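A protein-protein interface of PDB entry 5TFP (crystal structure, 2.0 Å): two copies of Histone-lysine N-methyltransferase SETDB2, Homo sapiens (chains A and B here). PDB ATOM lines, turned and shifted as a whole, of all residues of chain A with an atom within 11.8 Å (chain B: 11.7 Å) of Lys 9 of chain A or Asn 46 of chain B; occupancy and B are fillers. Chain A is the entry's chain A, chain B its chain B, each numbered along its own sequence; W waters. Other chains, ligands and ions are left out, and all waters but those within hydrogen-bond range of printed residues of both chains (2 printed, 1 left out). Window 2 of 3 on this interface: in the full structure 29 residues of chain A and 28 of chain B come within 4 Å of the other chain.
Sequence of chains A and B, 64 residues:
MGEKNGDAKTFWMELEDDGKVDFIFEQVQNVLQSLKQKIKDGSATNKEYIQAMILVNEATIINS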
ATOM      1  N   GLY A   6      -2.482   9.374 -11.619  1.00  0.00           N
ATOM      2  CA  GLY A   6      -2.354   9.942 -12.949  1.00  0.00           C
ATOM      3  C   GLY A   6      -0.903  10.039 -13.395  1.00  0.00           C
ATOM      4  O   GLY A   6      -0.622  10.469 -14.521  1.00  0.00           O
ATOM      5  N   ASP A   7       0.019   9.649 -12.510  1.00  0.00           N
ATOM      6  CA  ASP A   7       1.434   9.616 -12.866  1.00  0.00           C
ATOM      7  C   ASP A   7       1.708   8.467 -13.830  1.00  0.00           C
ATOM      8  O   ASP A   7       1.401   7.300 -13.555  1.00  0.00           O
ATOM      9  CB  ASP A   7       2.324   9.483 -11.649  1.00  0.00           C
ATOM     10  CG  ASP A   7       3.784   9.478 -12.021  1.00  0.00           C
ATOM     11  OD1 ASP A   7       4.345  10.575 -12.227  1.00  0.00           O
ATOM     12  OD2 ASP A   7       4.366   8.380 -12.138  1.00  0.00           O
ATOM     13  N   ALA A   8       2.295   8.812 -14.966  1.00  0.00           N
ATOM     14  CA  ALA A   8       2.317   7.895 -16.085  1.00  0.00           C
ATOM     15  C   ALA A   8       3.381   6.843 -15.854  1.00  0.00           C
ATOM     16  O   ALA A   8       3.189   5.688 -16.249  1.00  0.00           O
ATOM     17  CB  ALA A   8       2.549   8.636 -17.379  1.00  0.00           C
ATOM     18  N   LYS A   9       4.499   7.228 -15.228  1.00  0.00           N
ATOM     19  CA  LYS A   9       5.528   6.240 -14.870  1.00  0.00           C
ATOM     20  C   LYS A   9       4.955   5.161 -13.947  1.00  0.00           C
ATOM     21  O   LYS A   9       5.176   3.970 -14.169  1.00  0.00           O
ATOM     22  CB  LYS A   9       6.750   6.895 -14.191  1.00  0.00           C
ATOM     23  CG  LYS A   9       7.809   7.422 -15.158  1.00  0.00           C
ATOM     24  CD  LYS A   9       8.978   8.106 -14.457  1.00  0.00           C
ATOM     25  CE  LYS A   9       9.926   8.703 -15.493  1.00  0.00           C
ATOM     26  NZ  LYS A   9      10.992   9.561 -14.910  1.00  0.00           N
ATOM     27  N   THR A  10       4.218   5.584 -12.919  1.00  0.00           N
ATOM     28  CA  THR A  10       3.608   4.646 -11.975  1.00  0.00           C
ATOM     29  C   THR A  10       2.621   3.743 -12.683  1.00  0.00           C
ATOM     30  O   THR A  10       2.611   2.532 -12.461  1.00  0.00           O
ATOM     31  CB  THR A  10       2.877   5.361 -10.827  1.00  0.00           C
ATOM     32  OG1 THR A  10       3.815   6.128 -10.064  1.00  0.00           O
ATOM     33  CG2 THR A  10       2.209   4.347  -9.899  1.00  0.00           C
ATOM     34  N   PHE A  11       1.784   4.349 -13.525  1.00  0.00           N
ATOM     35  CA  PHE A  11       0.821   3.630 -14.353  1.00  0.00           C
ATOM     36  C   PHE A  11       1.486   2.460 -15.082  1.00  0.00           C
ATOM     37  O   PHE A  11       1.075   1.301 -14.946  1.00  0.00           O
ATOM     38  CB  PHE A  11       0.192   4.604 -15.353  1.00  0.00           C
ATOM     39  CG  PHE A  11      -0.745   3.968 -16.340  1.00  0.00           C
ATOM     40  CD1 PHE A  11      -2.069   3.747 -16.006  1.00  0.00           C
ATOM     41  CD2 PHE A  11      -0.306   3.619 -17.608  1.00  0.00           C
ATOM     42  CE1 PHE A  11      -2.943   3.182 -16.934  1.00  0.00           C
ATOM     43  CE2 PHE A  11      -1.162   3.051 -18.532  1.00  0.00           C
ATOM     44  CZ  PHE A  11      -2.482   2.828 -18.191  1.00  0.00           C
ATOM     45  N   TRP A  12       2.551   2.757 -15.815  1.00  0.00           N
ATOM     46  CA  TRP A  12       3.215   1.722 -16.601  1.00  0.00           C
ATOM     47  C   TRP A  12       4.043   0.741 -15.760  1.00  0.00           C
ATOM     48  O   TRP A  12       4.142  -0.439 -16.101  1.00  0.00           O
ATOM     49  CB  TRP A  12       4.083   2.370 -17.679  1.00  0.00           C
ATOM     50  CG  TRP A  12       3.210   2.869 -18.789  1.00  0.00           C
ATOM     51  CD1 TRP A  12       2.974   4.173 -19.132  1.00  0.00           C
ATOM     52  CD2 TRP A  12       2.417   2.071 -19.667  1.00  0.00           C
ATOM     53  NE1 TRP A  12       2.100   4.233 -20.193  1.00  0.00           N
ATOM     54  CE2 TRP A  12       1.738   2.957 -20.542  1.00  0.00           C
ATOM     55  CE3 TRP A  12       2.226   0.683 -19.819  1.00  0.00           C
ATOM     56  CZ2 TRP A  12       0.871   2.506 -21.552  1.00  0.00           C
ATOM     57  CZ3 TRP A  12       1.363   0.233 -20.824  1.00  0.00           C
ATOM     58  CH2 TRP A  12       0.689   1.140 -21.672  1.00  0.00           C
ATOM     59  N   MET A  13       4.616   1.218 -14.659  1.00  0.00           N
ATOM     60  CA  MET A  13       5.385   0.345 -13.767  1.00  0.00           C
ATOM     61  C   MET A  13       4.486  -0.740 -13.200  1.00  0.00           C
ATOM     62  O   MET A  13       4.861  -1.914 -13.147  1.00  0.00           O
ATOM     63  CB  MET A  13       6.035   1.153 -12.637  1.00  0.00           C
ATOM     64  CG  MET A  13       7.209   2.008 -13.142  1.00  0.00           C
ATOM     65  SD  MET A  13       8.169   3.072 -11.804  1.00  0.00           S
ATOM     66  CE  MET A  13       8.650   1.636 -10.568  1.00  0.00           C
ATOM     67  N   GLU A  14       3.284  -0.342 -12.795  1.00  0.00           N
ATOM     68  CA  GLU A  14       2.326  -1.271 -12.232  1.00  0.00           C
ATOM     69  C   GLU A  14       1.906  -2.313 -13.260  1.00  0.00           C
ATOM     70  O   GLU A  14       1.900  -3.516 -12.969  1.00  0.00           O
ATOM     71  CB  GLU A  14       1.108  -0.513 -11.693  1.00  0.00           C
ATOM     72  CG  GLU A  14       1.397   0.160 -10.350  1.00  0.00           C
ATOM     73  CD  GLU A  14       0.344   1.171  -9.931  1.00  0.00           C
ATOM     74  OE1 GLU A  14      -0.413   1.663 -10.799  1.00  0.00           O
ATOM     75  OE2 GLU A  14       0.286   1.482  -8.724  1.00  0.00           O
ATOM     76  N   LEU A  15       1.583  -1.853 -14.463  1.00  0.00           N
ATOM     77  CA  LEU A  15       1.202  -2.743 -15.551  1.00  0.00           C
ATOM     78  C   LEU A  15       2.347  -3.711 -15.870  1.00  0.00           C
ATOM     79  O   LEU A  15       2.137  -4.925 -16.011  1.00  0.00           O
ATOM     80  CB  LEU A  15       0.814  -1.931 -16.811  1.00  0.00           C
ATOM     81  CG  LEU A  15      -0.568  -1.258 -16.756  1.00  0.00           C
ATOM     82  CD1 LEU A  15      -0.771  -0.385 -17.993  1.00  0.00           C
ATOM     83  CD2 LEU A  15      -1.681  -2.294 -16.659  1.00  0.00           C
ATOM     84  N   GLU A  16       3.561  -3.161 -15.955  1.00  0.00           N
ATOM     85  CA  GLU A  16       4.748  -3.953 -16.278  1.00  0.00           C
ATOM     86  C   GLU A  16       5.020  -4.992 -15.201  1.00  0.00           C
ATOM     87  O   GLU A  16       5.238  -6.169 -15.512  1.00  0.00           O
ATOM     88  CB  GLU A  16       5.967  -3.042 -16.482  1.00  0.00           C
ATOM     89  CG  GLU A  16       7.046  -3.649 -17.379  1.00  0.00           C
ATOM     90  CD  GLU A  16       7.902  -4.654 -16.645  1.00  0.00           C
ATOM     91  OE1 GLU A  16       8.014  -4.499 -15.411  1.00  0.00           O
ATOM     92  OE2 GLU A  16       8.452  -5.588 -17.291  1.00  0.00           O
ATOM     93  N   ASP A  17       5.000  -4.570 -13.938  1.00  0.00           N
ATOM     94  CA  ASP A  17       5.224  -5.492 -12.821  1.00  0.00           C
ATOM     95  C   ASP A  17       4.147  -6.581 -12.790  1.00  0.00           C
ATOM     96  O   ASP A  17       4.408  -7.715 -12.378  1.00  0.00           O
ATOM     97  CB  ASP A  17       5.252  -4.740 -11.485  1.00  0.00           C
ATOM     98  CG  ASP A  17       5.691  -5.624 -10.322  1.00  0.00           C
ATOM     99  OD1 ASP A  17       6.593  -6.466 -10.513  1.00  0.00           O
ATOM    100  OD2 ASP A  17       5.136  -5.476  -9.214  1.00  0.00           O
ATOM    101  N   ASP A  18       2.943  -6.232 -13.240  1.00  0.00           N
ATOM    102  CA  ASP A  18       1.831  -7.190 -13.290  1.00  0.00           C
ATOM    103  C   ASP A  18       1.811  -8.048 -14.553  1.00  0.00           C
ATOM    104  O   ASP A  18       0.945  -8.903 -14.700  1.00  0.00           O
ATOM    105  CB  ASP A  18       0.485  -6.469 -13.181  1.00  0.00           C
ATOM    106  CG  ASP A  18       0.169  -6.029 -11.769  1.00  0.00           C
ATOM    107  OD1 ASP A  18       0.983  -6.303 -10.858  1.00  0.00           O
ATOM    108  OD2 ASP A  18      -0.904  -5.418 -11.568  1.00  0.00           O
ATOM    109  N   VAL A  21       1.577  -5.456 -19.913  1.00  0.00           N
ATOM    110  CA  VAL A  21       1.879  -4.484 -20.959  1.00  0.00           C
ATOM    111  C   VAL A  21       1.464  -5.022 -22.353  1.00  0.00           C
ATOM    112  O   VAL A  21       0.765  -4.331 -23.100  1.00  0.00           O
ATOM    113  CB  VAL A  21       3.367  -4.091 -20.950  1.00  0.00           C
ATOM    114  CG1 VAL A  21       3.676  -3.232 -22.164  1.00  0.00           C
ATOM    115  CG2 VAL A  21       3.708  -3.317 -19.654  1.00  0.00           C
ATOM    116  N   PHE A  25      -1.527  -3.342 -24.929  1.00  0.00           N
ATOM    117  CA  PHE A  25      -1.206  -2.931 -26.298  1.00  0.00           C
ATOM    118  C   PHE A  25      -1.975  -3.778 -27.342  1.00  0.00           C
ATOM    119  O   PHE A  25      -2.341  -3.251 -28.391  1.00  0.00           O
ATOM    120  CB  PHE A  25       0.321  -2.984 -26.530  1.00  0.00           C
ATOM    121  CG  PHE A  25       1.017  -1.717 -26.088  1.00  0.00           C
ATOM    122  CD1 PHE A  25       1.064  -0.606 -26.932  1.00  0.00           C
ATOM    123  CD2 PHE A  25       1.580  -1.614 -24.808  1.00  0.00           C
ATOM    124  CE1 PHE A  25       1.675   0.590 -26.526  1.00  0.00           C
ATOM    125  CE2 PHE A  25       2.196  -0.423 -24.391  1.00  0.00           C
ATOM    126  CZ  PHE A  25       2.245   0.686 -25.253  1.00  0.00           C
ATOM    127  N   GLU A  58      -2.542  11.988 -31.108  1.00  0.00           N
ATOM    128  CA  GLU A  58      -1.811  11.619 -29.894  1.00  0.00           C
ATOM    129  C   GLU A  58      -0.594  10.751 -30.235  1.00  0.00           C
ATOM    130  O   GLU A  58       0.420  10.799 -29.555  1.00  0.00           O
ATOM    131  CB  GLU A  58      -2.739  10.906 -28.906  1.00  0.00           C
ATOM    132  CG  GLU A  58      -3.702  11.897 -28.246  1.00  0.00           C
ATOM    133  CD  GLU A  58      -4.828  11.257 -27.465  1.00  0.00           C
ATOM    134  OE1 GLU A  58      -5.054  10.025 -27.595  1.00  0.00           O
ATOM    135  OE2 GLU A  58      -5.485  12.010 -26.704  1.00  0.00           O
ATOM    136  N   ILE A  62       2.021  14.425 -30.967  1.00  0.00           N
ATOM    137  CA  ILE A  62       2.685  14.393 -29.666  1.00  0.00           C
ATOM    138  C   ILE A  62       4.070  13.744 -29.797  1.00  0.00           C
ATOM    139  O   ILE A  62       4.213  12.721 -30.464  1.00  0.00           O
ATOM    140  CB  ILE A  62       1.847  13.623 -28.609  1.00  0.00           C
ATOM    141  CG1 ILE A  62       0.455  14.252 -28.449  1.00  0.00           C
ATOM    142  CG2 ILE A  62       2.581  13.570 -27.268  1.00  0.00           C
ATOM    143  CD1 ILE A  62       0.483  15.690 -27.942  1.00  0.00           C
ATOM    144  N   ASN A  63       5.072  14.364 -29.169  1.00  0.00           N
ATOM    145  CA  ASN A  63       6.448  13.865 -29.151  1.00  0.00           C
ATOM    146  C   ASN A  63       7.073  13.702 -30.534  1.00  0.00           C
ATOM    147  O   ASN A  63       8.052  12.969 -30.690  1.00  0.00           O
ATOM    148  CB  ASN A  63       6.537  12.524 -28.409  1.00  0.00           C
ATOM    149  CG  ASN A  63       6.270  12.659 -26.922  1.00  0.00           C
ATOM    150  OD1 ASN A  63       5.824  11.710 -26.266  1.00  0.00           O
ATOM    151  ND2 ASN A  63       6.541  13.846 -26.378  1.00  0.00           N
ATOM    152  N   LEU B  35       6.589   2.557 -28.563  1.00  0.00           N
ATOM    153  CA  LEU B  35       6.286   2.885 -27.156  1.00  0.00           C
ATOM    154  C   LEU B  35       6.264   1.633 -26.302  1.00  0.00           C
ATOM    155  O   LEU B  35       6.792   1.610 -25.191  1.00  0.00           O
ATOM    156  CB  LEU B  35       4.937   3.605 -27.028  1.00  0.00           C
ATOM    157  CG  LEU B  35       4.950   5.051 -27.563  1.00  0.00           C
ATOM    158  CD1 LEU B  35       3.518   5.612 -27.616  1.00  0.00           C
ATOM    159  CD2 LEU B  35       5.843   5.935 -26.704  1.00  0.00           C
ATOM    160  N   LYS B  38       9.890   0.407 -25.737  1.00  0.00           N
ATOM    161  CA  LYS B  38      10.598   1.285 -24.811  1.00  0.00           C
ATOM    162  C   LYS B  38      10.136   1.079 -23.388  1.00  0.00           C
ATOM    163  O   LYS B  38      10.963   1.038 -22.473  1.00  0.00           O
ATOM    164  CB  LYS B  38      10.409   2.757 -25.213  1.00  0.00           C
ATOM    165  CG  LYS B  38      11.205   3.125 -26.436  1.00  0.00           C
ATOM    166  CD  LYS B  38      10.757   4.459 -27.033  1.00  0.00           C
ATOM    167  CE  LYS B  38      11.651   4.833 -28.221  1.00  0.00           C
ATOM    168  NZ  LYS B  38      11.206   6.115 -28.859  1.00  0.00           N
ATOM    169  N   ILE B  39       8.822   0.924 -23.199  1.00  0.00           N
ATOM    170  CA  ILE B  39       8.272   0.626 -21.870  1.00  0.00           C
ATOM    171  C   ILE B  39       8.757  -0.722 -21.318  1.00  0.00           C
ATOM    172  O   ILE B  39       9.231  -0.796 -20.162  1.00  0.00           O
ATOM    173  CB  ILE B  39       6.729   0.665 -21.899  1.00  0.00           C
ATOM    174  CG1 ILE B  39       6.271   2.114 -22.026  1.00  0.00           C
ATOM    175  CG2 ILE B  39       6.112   0.041 -20.610  1.00  0.00           C
ATOM    176  CD1 ILE B  39       4.794   2.251 -22.557  1.00  0.00           C
ATOM    177  N   LYS B  40       8.669  -1.783 -22.120  1.00  0.00           N
ATOM    178  CA  LYS B  40       9.157  -3.091 -21.640  1.00  0.00           C
ATOM    179  C   LYS B  40      10.674  -3.103 -21.395  1.00  0.00           C
ATOM    180  O   LYS B  40      11.153  -3.793 -20.485  1.00  0.00           O
ATOM    181  CB  LYS B  40       8.776  -4.195 -22.625  1.00  0.00           C
ATOM    182  CG  LYS B  40       7.274  -4.424 -22.696  1.00  0.00           C
ATOM    183  CD  LYS B  40       6.890  -5.334 -23.834  1.00  0.00           C
ATOM    184  CE  LYS B  40       7.394  -6.733 -23.605  1.00  0.00           C
ATOM    185  NZ  LYS B  40       6.850  -7.616 -24.681  1.00  0.00           N
ATOM    186  N   GLY B  42      12.517  -0.503 -20.467  1.00  0.00           N
ATOM    187  CA  GLY B  42      12.924   0.445 -19.448  1.00  0.00           C
ATOM    188  C   GLY B  42      13.633   1.682 -20.000  1.00  0.00           C
ATOM    189  O   GLY B  42      14.227   2.434 -19.245  1.00  0.00           O
ATOM    190  N   SER B  43      13.567   1.902 -21.305  1.00  0.00           N
ATOM    191  CA  SER B  43      14.247   3.056 -21.896  1.00  0.00           C
ATOM    192  C   SER B  43      13.301   4.206 -22.246  1.00  0.00           C
ATOM    193  O   SER B  43      13.734   5.209 -22.812  1.00  0.00           O
ATOM    194  CB  SER B  43      15.011   2.631 -23.153  1.00  0.00           C
ATOM    195  OG  SER B  43      14.131   2.093 -24.125  1.00  0.00           O
ATOM    196  N   ALA B  44      12.012   4.066 -21.928  1.00  0.00           N
ATOM    197  CA  ALA B  44      11.046   5.117 -22.255  1.00  0.00           C
ATOM    198  C   ALA B  44      11.359   6.396 -21.483  1.00  0.00           C
ATOM    199  O   ALA B  44      11.770   6.343 -20.329  1.00  0.00           O
ATOM    200  CB  ALA B  44       9.624   4.659 -21.957  1.00  0.00           C
ATOM    201  N   THR B  45      11.181   7.549 -22.126  1.00  0.00           N
ATOM    202  CA  THR B  45      11.313   8.822 -21.416  1.00  0.00           C
ATOM    203  C   THR B  45      10.003   9.104 -20.709  1.00  0.00           C
ATOM    204  O   THR B  45       8.968   8.514 -21.013  1.00  0.00           O
ATOM    205  CB  THR B  45      11.591  10.033 -22.356  1.00  0.00           C
ATOM    206  OG1 THR B  45      10.461  10.205 -23.210  1.00  0.00           O
ATOM    207  CG2 THR B  45      12.861   9.848 -23.202  1.00  0.00           C
ATOM    208  N   ASN B  46      10.035  10.049 -19.798  1.00  0.00           N
ATOM    209  CA  ASN B  46       8.816  10.525 -19.199  1.00  0.00           C
ATOM    210  C   ASN B  46       7.728  10.944 -20.212  1.00  0.00           C
ATOM    211  O   ASN B  46       6.542  10.593 -20.060  1.00  0.00           O
ATOM    212  CB  ASN B  46       9.159  11.685 -18.279  1.00  0.00           C
ATOM    213  CG  ASN B  46       8.003  12.084 -17.426  1.00  0.00           C
ATOM    214  OD1 ASN B  46       7.565  13.235 -17.447  1.00  0.00           O
ATOM    215  ND2 ASN B  46       7.473  11.124 -16.681  1.00  0.00           N
ATOM    216  N   LYS B  47       8.109  11.694 -21.243  1.00  0.00           N
ATOM    217  CA  LYS B  47       7.111  12.115 -22.228  1.00  0.00           C
ATOM    218  C   LYS B  47       6.559  10.915 -22.983  1.00  0.00           C
ATOM    219  O   LYS B  47       5.396  10.921 -23.369  1.00  0.00           O
ATOM    220  CB  LYS B  47       7.681  13.145 -23.208  1.00  0.00           C
ATOM    221  CG  LYS B  47       8.104  14.455 -22.520  1.00  0.00           C
ATOM    222  CD  LYS B  47       8.181  15.649 -23.474  1.00  0.00           C
ATOM    223  CE  LYS B  47       8.461  16.944 -22.688  1.00  0.00           C
ATOM    224  NZ  LYS B  47       8.372  18.207 -23.494  1.00  0.00           N
ATOM    225  N   GLU B  48       7.365   9.874 -23.173  1.00  0.00           N
ATOM    226  CA  GLU B  48       6.838   8.675 -23.847  1.00  0.00           C
ATOM    227  C   GLU B  48       5.871   7.872 -22.950  1.00  0.00           C
ATOM    228  O   GLU B  48       4.871   7.336 -23.454  1.00  0.00           O
ATOM    229  CB  GLU B  48       7.991   7.784 -24.348  1.00  0.00           C
ATOM    230  CG  GLU B  48       8.784   8.463 -25.498  1.00  0.00           C
ATOM    231  CD  GLU B  48      10.140   7.814 -25.793  1.00  0.00           C
ATOM    232  OE1 GLU B  48      10.742   7.168 -24.893  1.00  0.00           O
ATOM    233  OE2 GLU B  48      10.599   7.941 -26.950  1.00  0.00           O
ATOM    234  N   TYR B  49       6.156   7.780 -21.647  1.00  0.00           N
ATOM    235  CA  TYR B  49       5.218   7.141 -20.705  1.00  0.00           C
ATOM    236  C   TYR B  49       3.869   7.846 -20.710  1.00  0.00           C
ATOM    237  O   TYR B  49       2.810   7.204 -20.760  1.00  0.00           O
ATOM    238  CB  TYR B  49       5.747   7.151 -19.278  1.00  0.00           C
ATOM    239  CG  TYR B  49       6.811   6.125 -18.985  1.00  0.00           C
ATOM    240  CD1 TYR B  49       6.552   4.753 -19.108  1.00  0.00           C
ATOM    241  CD2 TYR B  49       8.072   6.530 -18.546  1.00  0.00           C
ATOM    242  CE1 TYR B  49       7.534   3.813 -18.811  1.00  0.00           C
ATOM    243  CE2 TYR B  49       9.053   5.604 -18.259  1.00  0.00           C
ATOM    244  CZ  TYR B  49       8.780   4.249 -18.388  1.00  0.00           C
ATOM    245  OH  TYR B  49       9.793   3.361 -18.100  1.00  0.00           O
ATOM    246  N   ILE B  50       3.913   9.172 -20.645  1.00  0.00           N
ATOM    247  CA  ILE B  50       2.700   9.978 -20.729  1.00  0.00           C
ATOM    248  C   ILE B  50       1.959   9.745 -22.037  1.00  0.00           C
ATOM    249  O   ILE B  50       0.757   9.478 -22.036  1.00  0.00           O
ATOM    250  CB  ILE B  50       3.018  11.464 -20.591  1.00  0.00           C
ATOM    251  CG1 ILE B  50       3.523  11.722 -19.157  1.00  0.00           C
ATOM    252  CG2 ILE B  50       1.778  12.294 -20.965  1.00  0.00           C
ATOM    253  CD1 ILE B  50       4.304  13.018 -18.952  1.00  0.00           C
ATOM    254  N   GLN B  51       2.660   9.879 -23.154  1.00  0.00           N
ATOM    255  CA  GLN B  51       2.035   9.635 -24.453  1.00  0.00           C
ATOM    256  C   GLN B  51       1.362   8.255 -24.537  1.00  0.00           C
ATOM    257  O   GLN B  51       0.224   8.129 -25.005  1.00  0.00           O
ATOM    258  CB  GLN B  51       3.077   9.798 -25.574  1.00  0.00           C
ATOM    259  CG  GLN B  51       2.530   9.525 -26.974  1.00  0.00           C
ATOM    260  CD  GLN B  51       3.595   9.622 -28.032  1.00  0.00           C
ATOM    261  OE1 GLN B  51       4.770   9.395 -27.747  1.00  0.00           O
ATOM    262  NE2 GLN B  51       3.205   9.992 -29.255  1.00  0.00           N
ATOM    263  N   ALA B  52       2.049   7.211 -24.092  1.00  0.00           N
ATOM    264  CA  ALA B  52       1.466   5.867 -24.136  1.00  0.00           C
ATOM    265  C   ALA B  52       0.221   5.707 -23.236  1.00  0.00           C
ATOM    266  O   ALA B  52      -0.769   5.082 -23.626  1.00  0.00           O
ATOM    267  CB  ALA B  52       2.535   4.811 -23.744  1.00  0.00           C
ATOM    268  N   MET B  53       0.275   6.267 -22.037  1.00  0.00           N
ATOM    269  CA  MET B  53      -0.873   6.262 -21.144  1.00  0.00           C
ATOM    270  C   MET B  53      -2.077   6.920 -21.783  1.00  0.00           C
ATOM    271  O   MET B  53      -3.189   6.391 -21.742  1.00  0.00           O
ATOM    272  CB  MET B  53      -0.545   6.980 -19.827  1.00  0.00           C
ATOM    273  CG  MET B  53      -1.672   6.877 -18.827  1.00  0.00           C
ATOM    274  SD  MET B  53      -1.216   7.806 -17.204  1.00  0.00           S
ATOM    275  CE  MET B  53      -0.979   9.580 -17.941  1.00  0.00           C
ATOM    276  N   ILE B  54      -1.853   8.081 -22.389  1.00  0.00           N
ATOM    277  CA  ILE B  54      -2.948   8.817 -22.998  1.00  0.00           C
ATOM    278  C   ILE B  54      -3.523   8.041 -24.177  1.00  0.00           C
ATOM    279  O   ILE B  54      -4.728   7.981 -24.336  1.00  0.00           O
ATOM    280  CB  ILE B  54      -2.483  10.226 -23.439  1.00  0.00           C
ATOM    281  CG1 ILE B  54      -2.307  11.100 -22.182  1.00  0.00           C
ATOM    282  CG2 ILE B  54      -3.489  10.849 -24.395  1.00  0.00           C
ATOM    283  CD1 ILE B  54      -1.716  12.462 -22.449  1.00  0.00           C
ATOM    284  N   LEU B  55      -2.668   7.419 -24.990  1.00  0.00           N
ATOM    285  CA  LEU B  55      -3.166   6.609 -26.123  1.00  0.00           C
ATOM    286  C   LEU B  55      -4.014   5.416 -25.685  1.00  0.00           C
ATOM    287  O   LEU B  55      -5.070   5.134 -26.288  1.00  0.00           O
ATOM    288  CB  LEU B  55      -1.996   6.096 -26.981  1.00  0.00           C
ATOM    289  CG  LEU B  55      -1.340   7.095 -27.936  1.00  0.00           C
ATOM    290  CD1 LEU B  55       0.055   6.590 -28.366  1.00  0.00           C
ATOM    291  CD2 LEU B  55      -2.228   7.366 -29.173  1.00  0.00           C
ATOM    292  N   ASN B  57      -5.669   5.045 -22.872  1.00  0.00           N
ATOM    293  CA  ASN B  57      -6.916   5.498 -22.295  1.00  0.00           C
ATOM    294  C   ASN B  57      -7.885   6.017 -23.350  1.00  0.00           C
ATOM    295  O   ASN B  57      -9.095   5.917 -23.161  1.00  0.00           O
ATOM    296  CB  ASN B  57      -6.649   6.536 -21.206  1.00  0.00           C
ATOM    297  CG  ASN B  57      -6.190   5.878 -19.900  1.00  0.00           C
ATOM    298  OD1 ASN B  57      -6.984   5.245 -19.208  1.00  0.00           O
ATOM    299  ND2 ASN B  57      -4.908   5.989 -19.587  1.00  0.00           N
HETATM  300  O   HOH W   1       5.312  10.474 -31.879  1.00  0.00           O
HETATM  301  O   HOH W   2       9.967  -5.945 -19.523  1.00  0.00           O
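The indole nitrogen of Trp 12 of chain A lies within hydrogen-bond range of the backbone carbonyl oxygen of Tyr 49 of chain B (3.1 Å). The backbone carbonyl oxygen (O) of Glu 58 of chain A lies within hydrogen-bond range of the side-chain amide nitrogen (NE2) of Gln 51 of chain B (2.9 Å). O of Ile 62 of chain A sits at hydrogen-bond distance from NE2 of Gln 51 of chain B, at 3.2 Å. OD1 of Asn 63 of chain A sits close to O of Lys 47 of chain B, at 3.0 Å. The side-chain amide oxygen (OD1) of Asn 63 of chain A lies close to the side-chain amide oxygen (OE1) of Gln 51 of chain B. NE1 of Trp 12 of chain A lies close to N of Met 53 of chain B (3.3 Å).
The side-chain carboxylate of Asp 7 of chain A sits at hydrogen-bond distance from the backbone NH of Lys 9 of chain A (3.3 Å). The side-chain amino group (NZ) of Lys 38 of chain B is in salt-bridge range of the side-chain carboxylate (OE2) of Glu 48 of chain B, 2.7 Å away. O of Met 53 of chain B lies within hydrogen-bond range of ND2 of Asn 57 of chain B (2.8 Å).
Among the printed residues, pairs that only touch across the chains: Glu 58 of chain A with Ile 54 of chain B (3.3 Å), Lys 9 of chain A with Tyr 49 of chain B (3.5 Å), Gly 6 of chain A with Met 53 of chain B (3.6 Å), Ala 8 of chain A with Ile 50 of chain B (3.6 Å), Glu 58 of chain A with Leu 55 of chain B (3.6 Å), Trp 12 of chain A with Ala 52 of chain B (3.6 Å), Lys 9 of chain A with Asn 46 of chain B (3.6 Å), Ala 8 of chain A with Tyr 49 of chain B (3.7 Å), Ala 8 of chain A with Met 53 of chain B (3.7 Å), Trp 12 of chain A with Ile 39 of chain B (3.7 Å), Phe 11 of chain A with Met 53 of chain B (3.7 Å), Val 21 of chain A with Lys 40 of chain B (3.8 Å) and Asn 63 of chain A with Glu 48 of chain B (3.9 Å).
Of the printed residues of chain B, Lys 9 of chain A touches Asn 46 (3.6 Å) and Tyr 49 (3.5 Å). Of chain A, only Lys 9 (3.6 Å) comes within 4 Å of Asn 46 of chain B. No residue of chain B comes within 4 Å of Asp 7 of chain A. Of chain B, only Tyr 49, Ile 50 and Met 53 come within 4 Å of Ala 8 of chain A. No residue of chain A comes within 4 Å of Ala 44 of chain B. No residue of chain A comes within 4 Å of Thr 45 of chain B. Ile 50 of chain B touches just one residue of chain A: Ala 8 (3.6 Å). Printed residues of chain A within 4 Å of Met 53 of chain B: Gly 6 (3.6 Å), Ala 8 (3.7 Å), Phe 11 (3.7 Å) and Trp 12 (3.3 Å). Printed residues of chain A within 4 Å of Leu 55 of chain B: Glu 58. Of the printed residues of chain B, Val 21 of chain A touches Lys 40. Gly 42 of chain B touches none of the printed residues of chain A. The nearest residue of chain B that does not touch Lys 9 of chain A is Thr 45 of chain B (5.2 Å).
Of the 19 printed residues of chain B, 12 touch a printed residue of chain A. Of the 18 printed residues of chain A, 9 touch a printed residue of chain B. Hydrophobic or aromatic side chains of chain A that line the printed part of chain B: Ala 8, Phe 11, Trp 12, Val 21 and Ile 62. Among the printed residues, no Asp or Glu carboxylate lies within 4 Å of a Lys or Arg side-chain nitrogen of the other chain.
No position is printed for both chains.
Water W2 lies within hydrogen-bond range of the backbone carbonyl oxygen of Lys 40 of chain B (2.6 Å) and the side-chain carboxylate of Glu 16 of chain A (2.7 Å). Water W1 bridges the backbone carbonyl oxygen (O) of Ile 62 of chain A and the side-chain amide nitrogen (NE2) of Gln 51 of chain B.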
